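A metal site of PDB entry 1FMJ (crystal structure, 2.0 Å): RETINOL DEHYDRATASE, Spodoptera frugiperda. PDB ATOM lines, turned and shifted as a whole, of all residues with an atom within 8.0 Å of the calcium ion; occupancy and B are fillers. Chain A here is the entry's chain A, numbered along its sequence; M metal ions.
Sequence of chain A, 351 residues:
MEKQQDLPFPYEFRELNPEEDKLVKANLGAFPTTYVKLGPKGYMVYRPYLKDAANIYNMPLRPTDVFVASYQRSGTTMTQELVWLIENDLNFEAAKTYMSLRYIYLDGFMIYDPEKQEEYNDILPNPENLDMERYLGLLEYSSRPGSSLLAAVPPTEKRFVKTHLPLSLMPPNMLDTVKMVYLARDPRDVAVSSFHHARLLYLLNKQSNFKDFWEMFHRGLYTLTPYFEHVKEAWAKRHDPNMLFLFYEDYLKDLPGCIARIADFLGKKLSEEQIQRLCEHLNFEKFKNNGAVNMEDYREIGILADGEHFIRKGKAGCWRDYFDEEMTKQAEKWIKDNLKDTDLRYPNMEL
N of Asn 121 lies within hydrogen-bond range of OH of Tyr 135 (3.4 Å).
Of the 10 residues printed, 3 come within 4 Å of the calcium ion.
The calcium ion is bound by the side-chain amide oxygen (OD1) of Asn 121 (2.4 Å), the backbone carbonyl oxygen (O) of Glu 118 (2.5 Å) and the side-chain carboxylate (OD1) of Asp 122 (2.7 Å). The calcium ion has three donor atoms within binding distance.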
ATOM      1  N   LYS A 116       0.562 -11.499 -26.487  1.00  0.00           N
ATOM      2  CA  LYS A 116       0.273 -12.012 -25.155  1.00  0.00           C
ATOM      3  C   LYS A 116       0.355 -13.537 -25.058  1.00  0.00           C
ATOM      4  O   LYS A 116      -0.244 -14.148 -24.172  1.00  0.00           O
ATOM      5  CB  LYS A 116      -1.118 -11.546 -24.730  1.00  0.00           C
ATOM      6  CG  LYS A 116      -1.304 -10.047 -24.842  1.00  0.00           C
ATOM      7  CD  LYS A 116      -2.680  -9.614 -24.385  1.00  0.00           C
ATOM      8  CE  LYS A 116      -2.848  -8.116 -24.568  1.00  0.00           C
ATOM      9  NZ  LYS A 116      -4.139  -7.623 -24.018  1.00  0.00           N
ATOM     10  N   GLN A 117       1.115 -14.131 -25.962  1.00  0.00           N
ATOM     11  CA  GLN A 117       1.254 -15.583 -25.993  1.00  0.00           C
ATOM     12  C   GLN A 117       1.505 -16.217 -24.626  1.00  0.00           C
ATOM     13  O   GLN A 117       0.958 -17.276 -24.329  1.00  0.00           O
ATOM     14  CB  GLN A 117       2.382 -15.973 -26.953  1.00  0.00           C
ATOM     15  CG  GLN A 117       2.710 -17.462 -26.943  1.00  0.00           C
ATOM     16  CD  GLN A 117       3.717 -17.861 -28.005  1.00  0.00           C
ATOM     17  OE1 GLN A 117       4.311 -18.934 -27.933  1.00  0.00           O
ATOM     18  NE2 GLN A 117       3.894 -17.010 -29.004  1.00  0.00           N
ATOM     19  N   GLU A 118       2.318 -15.583 -23.797  1.00  0.00           N
ATOM     20  CA  GLU A 118       2.625 -16.137 -22.476  1.00  0.00           C
ATOM     21  C   GLU A 118       1.455 -16.154 -21.505  1.00  0.00           C
ATOM     22  O   GLU A 118       1.416 -16.977 -20.596  1.00  0.00           O
ATOM     23  CB  GLU A 118       3.790 -15.355 -21.816  1.00  0.00           C
ATOM     24  CG  GLU A 118       5.127 -15.421 -22.548  1.00  0.00           C
ATOM     25  CD  GLU A 118       5.242 -14.407 -23.685  1.00  0.00           C
ATOM     26  OE1 GLU A 118       6.353 -14.297 -24.252  1.00  0.00           O
ATOM     27  OE2 GLU A 118       4.238 -13.732 -24.004  1.00  0.00           O
ATOM     28  N   GLU A 119       0.499 -15.259 -21.718  1.00  0.00           N
ATOM     29  CA  GLU A 119      -0.664 -15.131 -20.842  1.00  0.00           C
ATOM     30  C   GLU A 119      -1.797 -16.140 -21.017  1.00  0.00           C
ATOM     31  O   GLU A 119      -2.603 -16.327 -20.107  1.00  0.00           O
ATOM     32  CB  GLU A 119      -1.243 -13.731 -20.992  1.00  0.00           C
ATOM     33  CG  GLU A 119      -0.247 -12.624 -20.674  1.00  0.00           C
ATOM     34  CD  GLU A 119      -0.765 -11.267 -21.046  1.00  0.00           C
ATOM     35  OE1 GLU A 119      -1.931 -10.964 -20.738  1.00  0.00           O
ATOM     36  OE2 GLU A 119      -0.001 -10.484 -21.667  1.00  0.00           O
ATOM     37  N   TYR A 120      -1.865 -16.810 -22.165  1.00  0.00           N
ATOM     38  CA  TYR A 120      -2.964 -17.733 -22.408  1.00  0.00           C
ATOM     39  C   TYR A 120      -3.009 -19.069 -21.687  1.00  0.00           C
ATOM     40  O   TYR A 120      -4.094 -19.535 -21.337  1.00  0.00           O
ATOM     41  CB  TYR A 120      -3.098 -17.968 -23.907  1.00  0.00           C
ATOM     42  CG  TYR A 120      -3.474 -16.723 -24.662  1.00  0.00           C
ATOM     43  CD1 TYR A 120      -2.512 -15.980 -25.329  1.00  0.00           C
ATOM     44  CD2 TYR A 120      -4.787 -16.286 -24.695  1.00  0.00           C
ATOM     45  CE1 TYR A 120      -2.858 -14.832 -26.030  1.00  0.00           C
ATOM     46  CE2 TYR A 120      -5.145 -15.133 -25.389  1.00  0.00           C
ATOM     47  CZ  TYR A 120      -4.172 -14.420 -26.048  1.00  0.00           C
ATOM     48  OH  TYR A 120      -4.522 -13.295 -26.755  1.00  0.00           O
ATOM     49  N   ASN A 121      -1.861 -19.689 -21.465  1.00  0.00           N
ATOM     50  CA  ASN A 121      -1.869 -20.977 -20.785  1.00  0.00           C
ATOM     51  C   ASN A 121      -2.188 -20.816 -19.313  1.00  0.00           C
ATOM     52  O   ASN A 121      -2.520 -21.780 -18.629  1.00  0.00           O
ATOM     53  CB  ASN A 121      -0.526 -21.689 -20.970  1.00  0.00           C
ATOM     54  CG  ASN A 121       0.634 -20.735 -20.923  1.00  0.00           C
ATOM     55  OD1 ASN A 121       0.955 -20.182 -19.870  1.00  0.00           O
ATOM     56  ND2 ASN A 121       1.275 -20.520 -22.077  1.00  0.00           N
ATOM     57  N   ASP A 122      -2.099 -19.577 -18.838  1.00  0.00           N
ATOM     58  CA  ASP A 122      -2.367 -19.276 -17.441  1.00  0.00           C
ATOM     59  C   ASP A 122      -3.862 -19.331 -17.116  1.00  0.00           C
ATOM     60  O   ASP A 122      -4.265 -19.283 -15.956  1.00  0.00           O
ATOM     61  CB  ASP A 122      -1.813 -17.896 -17.098  1.00  0.00           C
ATOM     62  CG  ASP A 122      -0.321 -17.779 -17.393  1.00  0.00           C
ATOM     63  OD1 ASP A 122       0.338 -18.826 -17.615  1.00  0.00           O
ATOM     64  OD2 ASP A 122       0.210 -16.644 -17.394  1.00  0.00           O
ATOM     65  N   ILE A 123      -4.698 -19.432 -18.147  1.00  0.00           N
ATOM     66  CA  ILE A 123      -6.142 -19.498 -17.935  1.00  0.00           C
ATOM     67  C   ILE A 123      -6.559 -20.943 -17.715  1.00  0.00           C
ATOM     68  O   ILE A 123      -7.721 -21.232 -17.435  1.00  0.00           O
ATOM     69  CB  ILE A 123      -6.907 -18.951 -19.170  1.00  0.00           C
ATOM     70  CG1 ILE A 123      -6.746 -19.897 -20.353  1.00  0.00           C
ATOM     71  CG2 ILE A 123      -6.415 -17.549 -19.515  1.00  0.00           C
ATOM     72  CD1 ILE A 123      -7.371 -19.395 -21.645  1.00  0.00           C
ATOM     73  N   PRO A 127      -1.753 -25.807 -16.623  1.00  0.00           N
ATOM     74  CA  PRO A 127      -0.994 -25.425 -17.815  1.00  0.00           C
ATOM     75  C   PRO A 127       0.103 -26.435 -18.161  1.00  0.00           C
ATOM     76  O   PRO A 127       0.627 -26.443 -19.271  1.00  0.00           O
ATOM     77  CB  PRO A 127      -0.406 -24.066 -17.442  1.00  0.00           C
ATOM     78  CG  PRO A 127      -1.382 -23.530 -16.430  1.00  0.00           C
ATOM     79  CD  PRO A 127      -1.670 -24.747 -15.597  1.00  0.00           C
ATOM     80  N   TYR A 135      -0.397 -27.508 -29.041  1.00  0.00           N
ATOM     81  CA  TYR A 135      -0.833 -26.236 -28.502  1.00  0.00           C
ATOM     82  C   TYR A 135      -0.180 -25.078 -29.259  1.00  0.00           C
ATOM     83  O   TYR A 135      -0.848 -24.131 -29.660  1.00  0.00           O
ATOM     84  CB  TYR A 135      -0.453 -26.148 -27.019  1.00  0.00           C
ATOM     85  CG  TYR A 135      -0.810 -24.834 -26.370  1.00  0.00           C
ATOM     86  CD1 TYR A 135      -2.141 -24.483 -26.155  1.00  0.00           C
ATOM     87  CD2 TYR A 135       0.182 -23.948 -25.959  1.00  0.00           C
ATOM     88  CE1 TYR A 135      -2.478 -23.274 -25.552  1.00  0.00           C
ATOM     89  CE2 TYR A 135      -0.138 -22.743 -25.354  1.00  0.00           C
ATOM     90  CZ  TYR A 135      -1.466 -22.410 -25.151  1.00  0.00           C
ATOM     91  OH  TYR A 135      -1.784 -21.228 -24.544  1.00  0.00           O
HETATM   92 CA    CA M   1       2.552 -18.533 -19.063  1.00  0.00          CA
